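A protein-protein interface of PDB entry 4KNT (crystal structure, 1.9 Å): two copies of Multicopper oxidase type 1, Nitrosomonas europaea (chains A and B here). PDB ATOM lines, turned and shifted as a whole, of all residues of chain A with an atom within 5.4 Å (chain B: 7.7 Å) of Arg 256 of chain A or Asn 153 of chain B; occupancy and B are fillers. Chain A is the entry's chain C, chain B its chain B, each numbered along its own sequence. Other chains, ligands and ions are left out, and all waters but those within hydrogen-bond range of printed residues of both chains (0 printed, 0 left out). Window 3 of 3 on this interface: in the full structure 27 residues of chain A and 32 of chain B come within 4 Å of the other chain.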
ATOM      1  N   ASN A 153       5.165 -14.544 -15.875  1.00  0.00           N
ATOM      2  CA  ASN A 153       4.163 -14.466 -16.942  1.00  0.00           C
ATOM      3  C   ASN A 153       3.934 -13.029 -17.430  1.00  0.00           C
ATOM      4  O   ASN A 153       2.825 -12.659 -17.826  1.00  0.00           O
ATOM      5  CB  ASN A 153       2.846 -15.126 -16.491  1.00  0.00           C
ATOM      6  CG  ASN A 153       1.968 -15.562 -17.657  1.00  0.00           C
ATOM      7  OD1 ASN A 153       2.458 -15.905 -18.733  1.00  0.00           O
ATOM      8  ND2 ASN A 153       0.655 -15.551 -17.438  1.00  0.00           N
ATOM      9  N   TRP A 155       4.500 -11.152 -20.139  1.00  0.00           N
ATOM     10  CA  TRP A 155       4.764 -11.053 -21.572  1.00  0.00           C
ATOM     11  C   TRP A 155       4.409  -9.671 -22.103  1.00  0.00           C
ATOM     12  O   TRP A 155       3.685  -8.916 -21.449  1.00  0.00           O
ATOM     13  CB  TRP A 155       4.025 -12.152 -22.351  1.00  0.00           C
ATOM     14  CG  TRP A 155       2.594 -12.372 -21.925  1.00  0.00           C
ATOM     15  CD1 TRP A 155       2.128 -13.349 -21.089  1.00  0.00           C
ATOM     16  CD2 TRP A 155       1.449 -11.606 -22.323  1.00  0.00           C
ATOM     17  NE1 TRP A 155       0.767 -13.235 -20.937  1.00  0.00           N
ATOM     18  CE2 TRP A 155       0.324 -12.173 -21.682  1.00  0.00           C
ATOM     19  CE3 TRP A 155       1.264 -10.490 -23.153  1.00  0.00           C
ATOM     20  CZ2 TRP A 155      -0.970 -11.667 -21.847  1.00  0.00           C
ATOM     21  CZ3 TRP A 155      -0.024  -9.984 -23.314  1.00  0.00           C
ATOM     22  CH2 TRP A 155      -1.124 -10.575 -22.664  1.00  0.00           C
ATOM     23  N   GLU A 198       0.761 -19.540 -21.257  1.00  0.00           N
ATOM     24  CA  GLU A 198      -0.646 -19.161 -21.351  1.00  0.00           C
ATOM     25  C   GLU A 198      -1.537 -20.173 -22.058  1.00  0.00           C
ATOM     26  O   GLU A 198      -1.065 -21.027 -22.814  1.00  0.00           O
ATOM     27  CB  GLU A 198      -0.798 -17.785 -22.023  1.00  0.00           C
ATOM     28  CG  GLU A 198      -0.297 -16.603 -21.189  1.00  0.00           C
ATOM     29  CD  GLU A 198      -1.311 -16.110 -20.165  1.00  0.00           C
ATOM     30  OE1 GLU A 198      -2.236 -16.872 -19.804  1.00  0.00           O
ATOM     31  OE2 GLU A 198      -1.180 -14.950 -19.718  1.00  0.00           O
ATOM     32  N   SER A 254      -9.604 -14.718 -24.923  1.00  0.00           N
ATOM     33  CA  SER A 254      -9.134 -13.988 -23.753  1.00  0.00           C
ATOM     34  C   SER A 254      -8.669 -12.648 -24.304  1.00  0.00           C
ATOM     35  O   SER A 254      -7.554 -12.535 -24.823  1.00  0.00           O
ATOM     36  CB  SER A 254      -7.989 -14.723 -23.053  1.00  0.00           C
ATOM     37  OG  SER A 254      -7.567 -14.031 -21.885  1.00  0.00           O
ATOM     38  N   MET A 255      -9.546 -11.646 -24.220  1.00  0.00           N
ATOM     39  CA  MET A 255      -9.360 -10.385 -24.952  1.00  0.00           C
ATOM     40  C   MET A 255      -8.006  -9.698 -24.795  1.00  0.00           C
ATOM     41  O   MET A 255      -7.523  -9.076 -25.740  1.00  0.00           O
ATOM     42  CB  MET A 255     -10.501  -9.395 -24.683  1.00  0.00           C
ATOM     43  CG  MET A 255     -11.805  -9.686 -25.440  1.00  0.00           C
ATOM     44  SD  MET A 255     -11.658 -10.165 -27.186  1.00  0.00           S
ATOM     45  CE  MET A 255     -10.883  -8.749 -27.935  1.00  0.00           C
ATOM     46  N   ARG A 256      -7.397  -9.810 -23.615  1.00  0.00           N
ATOM     47  CA  ARG A 256      -6.067  -9.231 -23.403  1.00  0.00           C
ATOM     48  C   ARG A 256      -5.021  -9.896 -24.306  1.00  0.00           C
ATOM     49  O   ARG A 256      -4.067  -9.244 -24.718  1.00  0.00           O
ATOM     50  CB  ARG A 256      -5.652  -9.262 -21.923  1.00  0.00           C
ATOM     51  CG  ARG A 256      -5.389 -10.648 -21.340  1.00  0.00           C
ATOM     52  CD  ARG A 256      -5.235 -10.597 -19.821  1.00  0.00           C
ATOM     53  NE  ARG A 256      -3.974  -9.986 -19.412  1.00  0.00           N
ATOM     54  CZ  ARG A 256      -2.914 -10.650 -18.961  1.00  0.00           C
ATOM     55  NH1 ARG A 256      -2.935 -11.970 -18.842  1.00  0.00           N
ATOM     56  NH2 ARG A 256      -1.823  -9.984 -18.624  1.00  0.00           N
ATOM     57  N   HIS A 257      -5.214 -11.180 -24.620  1.00  0.00           N
ATOM     58  CA  HIS A 257      -4.350 -11.880 -25.580  1.00  0.00           C
ATOM     59  C   HIS A 257      -4.614 -11.395 -27.005  1.00  0.00           C
ATOM     60  O   HIS A 257      -3.673 -11.091 -27.746  1.00  0.00           O
ATOM     61  CB  HIS A 257      -4.536 -13.406 -25.534  1.00  0.00           C
ATOM     62  CG  HIS A 257      -4.187 -14.039 -24.221  1.00  0.00           C
ATOM     63  ND1 HIS A 257      -4.422 -15.373 -23.960  1.00  0.00           N
ATOM     64  CD2 HIS A 257      -3.634 -13.530 -23.094  1.00  0.00           C
ATOM     65  CE1 HIS A 257      -4.023 -15.660 -22.734  1.00  0.00           C
ATOM     66  NE2 HIS A 257      -3.540 -14.560 -22.187  1.00  0.00           N
ATOM     67  N   ALA A 258      -5.892 -11.342 -27.388  1.00  0.00           N
ATOM     68  CA  ALA A 258      -6.290 -10.862 -28.715  1.00  0.00           C
ATOM     69  C   ALA A 258      -5.751  -9.459 -28.998  1.00  0.00           C
ATOM     70  O   ALA A 258      -5.121  -9.234 -30.026  1.00  0.00           O
ATOM     71  CB  ALA A 258      -7.814 -10.897 -28.875  1.00  0.00           C
ATOM     72  N   HIS A 259      -5.980  -8.525 -28.072  1.00  0.00           N
ATOM     73  CA  HIS A 259      -5.524  -7.140 -28.256  1.00  0.00           C
ATOM     74  C   HIS A 259      -4.000  -6.998 -28.265  1.00  0.00           C
ATOM     75  O   HIS A 259      -3.473  -5.982 -28.726  1.00  0.00           O
ATOM     76  CB  HIS A 259      -6.125  -6.213 -27.195  1.00  0.00           C
ATOM     77  CG  HIS A 259      -7.603  -6.020 -27.323  1.00  0.00           C
ATOM     78  ND1 HIS A 259      -8.211  -5.651 -28.504  1.00  0.00           N
ATOM     79  CD2 HIS A 259      -8.594  -6.121 -26.406  1.00  0.00           C
ATOM     80  CE1 HIS A 259      -9.513  -5.543 -28.311  1.00  0.00           C
ATOM     81  NE2 HIS A 259      -9.771  -5.823 -27.046  1.00  0.00           N
ATOM     82  N   SER A 260      -3.304  -8.016 -27.759  1.00  0.00           N
ATOM     83  CA  SER A 260      -1.841  -8.015 -27.702  1.00  0.00           C
ATOM     84  C   SER A 260      -1.196  -8.674 -28.928  1.00  0.00           C
ATOM     85  O   SER A 260       0.028  -8.791 -28.997  1.00  0.00           O
ATOM     86  CB  SER A 260      -1.355  -8.695 -26.420  1.00  0.00           C
ATOM     87  OG  SER A 260      -1.831  -8.007 -25.276  1.00  0.00           O
ATOM     88  N   ILE B 105     -12.415  -5.682 -25.348  1.00  0.00           N
ATOM     89  CA  ILE B 105     -12.155  -5.909 -23.925  1.00  0.00           C
ATOM     90  C   ILE B 105     -12.988  -4.967 -23.038  1.00  0.00           C
ATOM     91  O   ILE B 105     -13.576  -5.401 -22.046  1.00  0.00           O
ATOM     92  CB  ILE B 105     -10.634  -5.828 -23.582  1.00  0.00           C
ATOM     93  CG1 ILE B 105     -10.355  -6.449 -22.202  1.00  0.00           C
ATOM     94  CG2 ILE B 105     -10.095  -4.389 -23.718  1.00  0.00           C
ATOM     95  CD1 ILE B 105      -8.878  -6.668 -21.893  1.00  0.00           C
ATOM     96  N   GLU B 139     -15.721 -10.553 -15.504  1.00  0.00           N
ATOM     97  CA  GLU B 139     -14.899  -9.810 -14.552  1.00  0.00           C
ATOM     98  C   GLU B 139     -15.390  -8.372 -14.454  1.00  0.00           C
ATOM     99  O   GLU B 139     -15.691  -7.739 -15.466  1.00  0.00           O
ATOM    100  CB  GLU B 139     -13.421  -9.813 -14.946  1.00  0.00           C
ATOM    101  CG  GLU B 139     -12.795 -11.186 -15.108  1.00  0.00           C
ATOM    102  CD  GLU B 139     -12.538 -11.532 -16.562  1.00  0.00           C
ATOM    103  OE1 GLU B 139     -11.952 -10.696 -17.282  1.00  0.00           O
ATOM    104  OE2 GLU B 139     -12.908 -12.647 -16.977  1.00  0.00           O
ATOM    105  N   TYR B 141     -14.411  -4.571 -13.427  1.00  0.00           N
ATOM    106  CA  TYR B 141     -13.252  -3.705 -13.261  1.00  0.00           C
ATOM    107  C   TYR B 141     -13.683  -2.407 -12.600  1.00  0.00           C
ATOM    108  O   TYR B 141     -14.664  -1.793 -13.014  1.00  0.00           O
ATOM    109  CB  TYR B 141     -12.569  -3.455 -14.613  1.00  0.00           C
ATOM    110  CG  TYR B 141     -11.965  -4.715 -15.194  1.00  0.00           C
ATOM    111  CD1 TYR B 141     -10.626  -5.037 -14.972  1.00  0.00           C
ATOM    112  CD2 TYR B 141     -12.741  -5.604 -15.940  1.00  0.00           C
ATOM    113  CE1 TYR B 141     -10.070  -6.206 -15.488  1.00  0.00           C
ATOM    114  CE2 TYR B 141     -12.195  -6.774 -16.460  1.00  0.00           C
ATOM    115  CZ  TYR B 141     -10.864  -7.068 -16.228  1.00  0.00           C
ATOM    116  OH  TYR B 141     -10.327  -8.227 -16.739  1.00  0.00           O
ATOM    117  N   LYS B 147      -8.487   1.078 -19.364  1.00  0.00           N
ATOM    118  CA  LYS B 147      -8.213  -0.002 -20.312  1.00  0.00           C
ATOM    119  C   LYS B 147      -6.910  -0.742 -20.005  1.00  0.00           C
ATOM    120  O   LYS B 147      -6.791  -1.936 -20.289  1.00  0.00           O
ATOM    121  CB  LYS B 147      -8.207   0.538 -21.744  1.00  0.00           C
ATOM    122  CG  LYS B 147      -9.599   0.888 -22.262  1.00  0.00           C
ATOM    123  CD  LYS B 147      -9.556   1.585 -23.616  1.00  0.00           C
ATOM    124  CE  LYS B 147      -9.390   3.088 -23.465  1.00  0.00           C
ATOM    125  NZ  LYS B 147      -9.211   3.745 -24.789  1.00  0.00           N
ATOM    126  N   THR B 148      -5.948  -0.030 -19.419  1.00  0.00           N
ATOM    127  CA  THR B 148      -4.675  -0.621 -18.993  1.00  0.00           C
ATOM    128  C   THR B 148      -4.877  -1.711 -17.937  1.00  0.00           C
ATOM    129  O   THR B 148      -4.312  -2.802 -18.052  1.00  0.00           O
ATOM    130  CB  THR B 148      -3.698   0.466 -18.475  1.00  0.00           C
ATOM    131  OG1 THR B 148      -3.374   1.350 -19.550  1.00  0.00           O
ATOM    132  CG2 THR B 148      -2.411  -0.149 -17.932  1.00  0.00           C
ATOM    133  N   ALA B 149      -5.687  -1.417 -16.921  1.00  0.00           N
ATOM    134  CA  ALA B 149      -5.993  -2.391 -15.872  1.00  0.00           C
ATOM    135  C   ALA B 149      -6.668  -3.637 -16.454  1.00  0.00           C
ATOM    136  O   ALA B 149      -6.395  -4.757 -16.016  1.00  0.00           O
ATOM    137  CB  ALA B 149      -6.859  -1.764 -14.787  1.00  0.00           C
ATOM    138  N   MET B 150      -7.538  -3.428 -17.443  1.00  0.00           N
ATOM    139  CA  MET B 150      -8.204  -4.526 -18.150  1.00  0.00           C
ATOM    140  C   MET B 150      -7.201  -5.386 -18.920  1.00  0.00           C
ATOM    141  O   MET B 150      -7.255  -6.617 -18.857  1.00  0.00           O
ATOM    142  CB  MET B 150      -9.285  -3.987 -19.094  1.00  0.00           C
ATOM    143  CG  MET B 150     -10.454  -3.320 -18.379  1.00  0.00           C
ATOM    144  SD  MET B 150     -11.597  -2.539 -19.532  1.00  0.00           S
ATOM    145  CE  MET B 150     -12.795  -1.828 -18.408  1.00  0.00           C
ATOM    146  N   MET B 151      -6.281  -4.730 -19.624  1.00  0.00           N
ATOM    147  CA  MET B 151      -5.222  -5.416 -20.368  1.00  0.00           C
ATOM    148  C   MET B 151      -4.288  -6.200 -19.448  1.00  0.00           C
ATOM    149  O   MET B 151      -3.740  -7.232 -19.837  1.00  0.00           O
ATOM    150  CB  MET B 151      -4.418  -4.418 -21.210  1.00  0.00           C
ATOM    151  CG  MET B 151      -5.160  -3.902 -22.436  1.00  0.00           C
ATOM    152  SD  MET B 151      -5.602  -5.216 -23.592  1.00  0.00           S
ATOM    153  CE  MET B 151      -4.000  -5.586 -24.312  1.00  0.00           C
ATOM    154  N   GLN B 152      -4.126  -5.706 -18.224  1.00  0.00           N
ATOM    155  CA  GLN B 152      -3.274  -6.348 -17.228  1.00  0.00           C
ATOM    156  C   GLN B 152      -4.044  -7.327 -16.337  1.00  0.00           C
ATOM    157  O   GLN B 152      -3.476  -7.903 -15.404  1.00  0.00           O
ATOM    158  CB  GLN B 152      -2.543  -5.288 -16.395  1.00  0.00           C
ATOM    159  CG  GLN B 152      -1.477  -4.540 -17.198  1.00  0.00           C
ATOM    160  CD  GLN B 152      -0.947  -3.299 -16.508  1.00  0.00           C
ATOM    161  OE1 GLN B 152      -1.342  -2.970 -15.389  1.00  0.00           O
ATOM    162  NE2 GLN B 152      -0.046  -2.592 -17.186  1.00  0.00           N
ATOM    163  N   ASN B 153      -5.331  -7.514 -16.640  1.00  0.00           N
ATOM    164  CA  ASN B 153      -6.186  -8.480 -15.943  1.00  0.00           C
ATOM    165  C   ASN B 153      -6.355  -8.154 -14.450  1.00  0.00           C
ATOM    166  O   ASN B 153      -6.460  -9.049 -13.606  1.00  0.00           O
ATOM    167  CB  ASN B 153      -5.648  -9.910 -16.147  1.00  0.00           C
ATOM    168  CG  ASN B 153      -6.691 -10.981 -15.882  1.00  0.00           C
ATOM    169  OD1 ASN B 153      -7.882 -10.794 -16.140  1.00  0.00           O
ATOM    170  ND2 ASN B 153      -6.241 -12.120 -15.369  1.00  0.00           N
ATOM    171  N   LYS B 154      -6.381  -6.863 -14.133  1.00  0.00           N
ATOM    172  CA  LYS B 154      -6.496  -6.413 -12.748  1.00  0.00           C
ATOM    173  C   LYS B 154      -7.947  -6.092 -12.395  1.00  0.00           C
ATOM    174  O   LYS B 154      -8.310  -4.934 -12.182  1.00  0.00           O
ATOM    175  CB  LYS B 154      -5.572  -5.218 -12.488  1.00  0.00           C
ATOM    176  CG  LYS B 154      -4.095  -5.579 -12.536  1.00  0.00           C
ATOM    177  CD  LYS B 154      -3.213  -4.347 -12.539  1.00  0.00           C
ATOM    178  CE  LYS B 154      -1.740  -4.738 -12.485  1.00  0.00           C
ATOM    179  NZ  LYS B 154      -0.861  -3.558 -12.712  1.00  0.00           N
ATOM    180  N   TRP B 155      -8.770  -7.136 -12.355  1.00  0.00           N
ATOM    181  CA  TRP B 155     -10.185  -7.003 -12.017  1.00  0.00           C
ATOM    182  C   TRP B 155     -10.379  -6.829 -10.520  1.00  0.00           C
ATOM    183  O   TRP B 155      -9.486  -7.148  -9.733  1.00  0.00           O
ATOM    184  CB  TRP B 155     -10.995  -8.201 -12.540  1.00  0.00           C
ATOM    185  CG  TRP B 155     -10.351  -9.553 -12.325  1.00  0.00           C
ATOM    186  CD1 TRP B 155      -9.622 -10.268 -13.235  1.00  0.00           C
ATOM    187  CD2 TRP B 155     -10.394 -10.348 -11.133  1.00  0.00           C
ATOM    188  NE1 TRP B 155      -9.203 -11.453 -12.683  1.00  0.00           N
ATOM    189  CE2 TRP B 155      -9.663 -11.531 -11.394  1.00  0.00           C
ATOM    190  CE3 TRP B 155     -10.976 -10.177  -9.868  1.00  0.00           C
ATOM    191  CZ2 TRP B 155      -9.496 -12.537 -10.438  1.00  0.00           C
ATOM    192  CZ3 TRP B 155     -10.808 -11.178  -8.915  1.00  0.00           C
ATOM    193  CH2 TRP B 155     -10.073 -12.343  -9.208  1.00  0.00           C
ATOM    194  N   SER B 156     -11.537  -6.300 -10.138  1.00  0.00           N
ATOM    195  CA  SER B 156     -11.872  -6.125  -8.730  1.00  0.00           C
ATOM    196  C   SER B 156     -12.748  -7.268  -8.235  1.00  0.00           C
ATOM    197  O   SER B 156     -12.603  -7.723  -7.103  1.00  0.00           O
ATOM    198  CB  SER B 156     -12.562  -4.781  -8.503  1.00  0.00           C
ATOM    199  OG  SER B 156     -11.751  -3.721  -8.976  1.00  0.00           O
ATOM    200  N   GLY B 195     -16.027 -13.313 -19.907  1.00  0.00           N
ATOM    201  CA  GLY B 195     -14.672 -12.818 -19.682  1.00  0.00           C
ATOM    202  C   GLY B 195     -14.682 -11.385 -19.174  1.00  0.00           C
ATOM    203  O   GLY B 195     -15.384 -11.085 -18.211  1.00  0.00           O
ATOM    204  N   PRO B 196     -13.948 -10.474 -19.844  1.00  0.00           N
ATOM    205  CA  PRO B 196     -13.248 -10.652 -21.125  1.00  0.00           C
ATOM    206  C   PRO B 196     -12.000 -11.542 -21.114  1.00  0.00           C
ATOM    207  O   PRO B 196     -11.610 -12.046 -22.173  1.00  0.00           O
ATOM    208  CB  PRO B 196     -12.851  -9.220 -21.511  1.00  0.00           C
ATOM    209  CG  PRO B 196     -12.799  -8.475 -20.214  1.00  0.00           C
ATOM    210  CD  PRO B 196     -13.903  -9.070 -19.389  1.00  0.00           C
ATOM    211  N   ASN B 197     -11.390 -11.737 -19.944  1.00  0.00           N
ATOM    212  CA  ASN B 197     -10.068 -12.373 -19.867  1.00  0.00           C
ATOM    213  C   ASN B 197     -10.006 -13.780 -19.277  1.00  0.00           C
ATOM    214  O   ASN B 197      -9.252 -14.622 -19.765  1.00  0.00           O
ATOM    215  CB  ASN B 197      -9.093 -11.490 -19.077  1.00  0.00           C
ATOM    216  CG  ASN B 197      -8.822 -10.157 -19.748  1.00  0.00           C
ATOM    217  OD1 ASN B 197      -8.817 -10.042 -20.981  1.00  0.00           O
ATOM    218  ND2 ASN B 197      -8.581  -9.136 -18.932  1.00  0.00           N
ATOM    219  N   GLU B 198     -10.777 -14.023 -18.222  1.00  0.00           N
ATOM    220  CA  GLU B 198     -10.548 -15.181 -17.358  1.00  0.00           C
ATOM    221  C   GLU B 198     -11.310 -16.442 -17.746  1.00  0.00           C
ATOM    222  O   GLU B 198     -12.310 -16.397 -18.465  1.00  0.00           O
ATOM    223  CB  GLU B 198     -10.844 -14.833 -15.891  1.00  0.00           C
ATOM    224  CG  GLU B 198      -9.934 -13.760 -15.290  1.00  0.00           C
ATOM    225  CD  GLU B 198      -8.590 -14.291 -14.813  1.00  0.00           C
ATOM    226  OE1 GLU B 198      -7.810 -14.802 -15.644  1.00  0.00           O
ATOM    227  OE2 GLU B 198      -8.292 -14.163 -13.608  1.00  0.00           O
ATOM    228  N   LEU B 199     -10.783 -17.559 -17.257  1.00  0.00           N
ATOM    229  CA  LEU B 199     -11.331 -18.898 -17.411  1.00  0.00           C
ATOM    230  C   LEU B 199     -12.246 -19.205 -16.221  1.00  0.00           C
ATOM    231  O   LEU B 199     -12.023 -18.670 -15.133  1.00  0.00           O
ATOM    232  CB  LEU B 199     -10.147 -19.861 -17.396  1.00  0.00           C
ATOM    233  CG  LEU B 199     -10.286 -21.365 -17.569  1.00  0.00           C
ATOM    234  CD1 LEU B 199     -10.765 -21.642 -18.960  1.00  0.00           C
ATOM    235  CD2 LEU B 199      -8.935 -22.021 -17.323  1.00  0.00           C
ATOM    236  N   ARG B 256      -9.878 -17.809  -5.930  1.00  0.00           N
ATOM    237  CA  ARG B 256      -9.794 -16.345  -5.971  1.00  0.00           C
ATOM    238  C   ARG B 256     -10.964 -15.710  -6.733  1.00  0.00           C
ATOM    239  O   ARG B 256     -11.373 -14.591  -6.418  1.00  0.00           O
ATOM    240  CB  ARG B 256      -8.437 -15.865  -6.505  1.00  0.00           C
ATOM    241  CG  ARG B 256      -8.163 -16.168  -7.974  1.00  0.00           C
ATOM    242  CD  ARG B 256      -6.701 -15.922  -8.318  1.00  0.00           C
ATOM    243  NE  ARG B 256      -6.382 -14.498  -8.390  1.00  0.00           N
ATOM    244  CZ  ARG B 256      -6.297 -13.797  -9.515  1.00  0.00           C
ATOM    245  NH1 ARG B 256      -6.507 -14.371 -10.690  1.00  0.00           N
ATOM    246  NH2 ARG B 256      -6.001 -12.509  -9.464  1.00  0.00           N
ATOM    247  N   HIS B 257     -11.494 -16.423  -7.730  1.00  0.00           N
ATOM    248  CA  HIS B 257     -12.692 -15.978  -8.450  1.00  0.00           C
ATOM    249  C   HIS B 257     -13.935 -16.122  -7.571  1.00  0.00           C
ATOM    250  O   HIS B 257     -14.717 -15.179  -7.442  1.00  0.00           O
ATOM    251  CB  HIS B 257     -12.906 -16.749  -9.763  1.00  0.00           C
ATOM    252  CG  HIS B 257     -11.808 -16.581 -10.770  1.00  0.00           C
ATOM    253  ND1 HIS B 257     -11.773 -17.294 -11.949  1.00  0.00           N
ATOM    254  CD2 HIS B 257     -10.699 -15.803 -10.769  1.00  0.00           C
ATOM    255  CE1 HIS B 257     -10.698 -16.952 -12.638  1.00  0.00           C
ATOM    256  NE2 HIS B 257     -10.029 -16.049 -11.943  1.00  0.00           N
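Arg 256 of chain A touches Asn 153 of chain B, but with the chains exchanged Asn 153 of chain A does not touch Arg 256 of chain B (9.9 Å).
5 positions are printed for both chains.
The backbone carbonyl oxygen (O) of Met 150 of chain B lies within hydrogen-bond range of the side-chain amide nitrogen (ND2) of Asn 197 of chain B, 2.8 Å away.
The side-chain hydroxyl (OH) of Tyr 141 of chain B sits at hydrogen-bond distance from the side-chain amide nitrogen (ND2) of Asn 197 of chain B, 2.9 Å away.
The side-chain amide oxygen of Asn 153 of chain B sits close to the side-chain amide nitrogen of Asn 197 of chain B (3.3 Å).
The backbone carbonyl oxygen (O) of Arg 256 of chain A lies within hydrogen-bond range of the side-chain hydroxyl (OG) of Ser 260 of chain A, at 2.6 Å.
OE2 of Glu 198 of chain A is in salt-bridge range of NH1 of Arg 256 of chain A, at 3.6 Å.
The side-chain carboxylate (OE1) of Glu 198 of chain B sits at hydrogen-bond distance from the side-chain amide nitrogen (ND2) of Asn 153 of chain B (3.1 Å).
Among the printed residues, pairs that only touch across the chains: Ser 254 of chain A with Pro 196 of chain B (3.5 Å), Met 255 of chain A with Ile 105 of chain B (3.7 Å), Met 255 of chain A with Asn 197 of chain B (3.7 Å), Arg 256 of chain A with Ile 105 of chain B (3.9 Å), Arg 256 of chain A with Asn 153 of chain B (3.7 Å), His 259 of chain A with Met 151 of chain B (3.6 Å) and Ser 260 of chain A with Met 151 of chain B (3.4 Å).
O of Pro 196 of chain B sits at hydrogen-bond distance from N of Met 255 of chain A (2.9 Å).
N of Arg 256 of chain A lies within hydrogen-bond range of OD1 of Asn 197 of chain B (3.0 Å).
O of Asn 197 of chain B lies within hydrogen-bond range of OG of Ser 254 of chain A.
A ring nitrogen (NE2) of His 259 of chain A is in hydrogen-bond range of the backbone NH (N) of Ile 105 of chain B, at 3.1 Å.
O of Met 151 of chain B is in hydrogen-bond range of NE of Arg 256 of chain A (2.8 Å).
Printed residues of chain B within 4 Å of Ser 254 of chain A: Pro 196 (3.5 Å) and Asn 197 (2.8 Å).
Arg 256 of chain A touches four residues of chain B.
Of the printed residues of chain B, His 259 of chain A touches Ile 105 (3.1 Å) and Met 151 (3.6 Å).
Printed residues of chain B within 4 Å of Ser 260 of chain A: Met 151 (3.4 Å).
Tyr 141 of chain B touches none of the printed residues of chain A.
Printed residues of chain A within 4 Å of Met 151 of chain B: Arg 256, His 259 and Ser 260.
Asn 153 of chain B touches just one residue of chain A: Arg 256 (3.7 Å).
The nearest residue of chain B that does not touch Arg 256 of chain A is Gln 152 of chain B (4.1 Å).
The nearest printed residue of chain B that does not touch Ser 254 of chain A is Glu 198 of chain B (4.9 Å).
Of the 20 printed residues of chain B, 5 touch a printed residue of chain A.
Hydrophobic or aromatic side chains of chain B that line the printed part of chain A: Ile 105, Met 151 and Pro 196.
Among the printed residues, no Asp or Glu carboxylate lies within 4 Å of a Lys or Arg side-chain nitrogen of the other chain.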
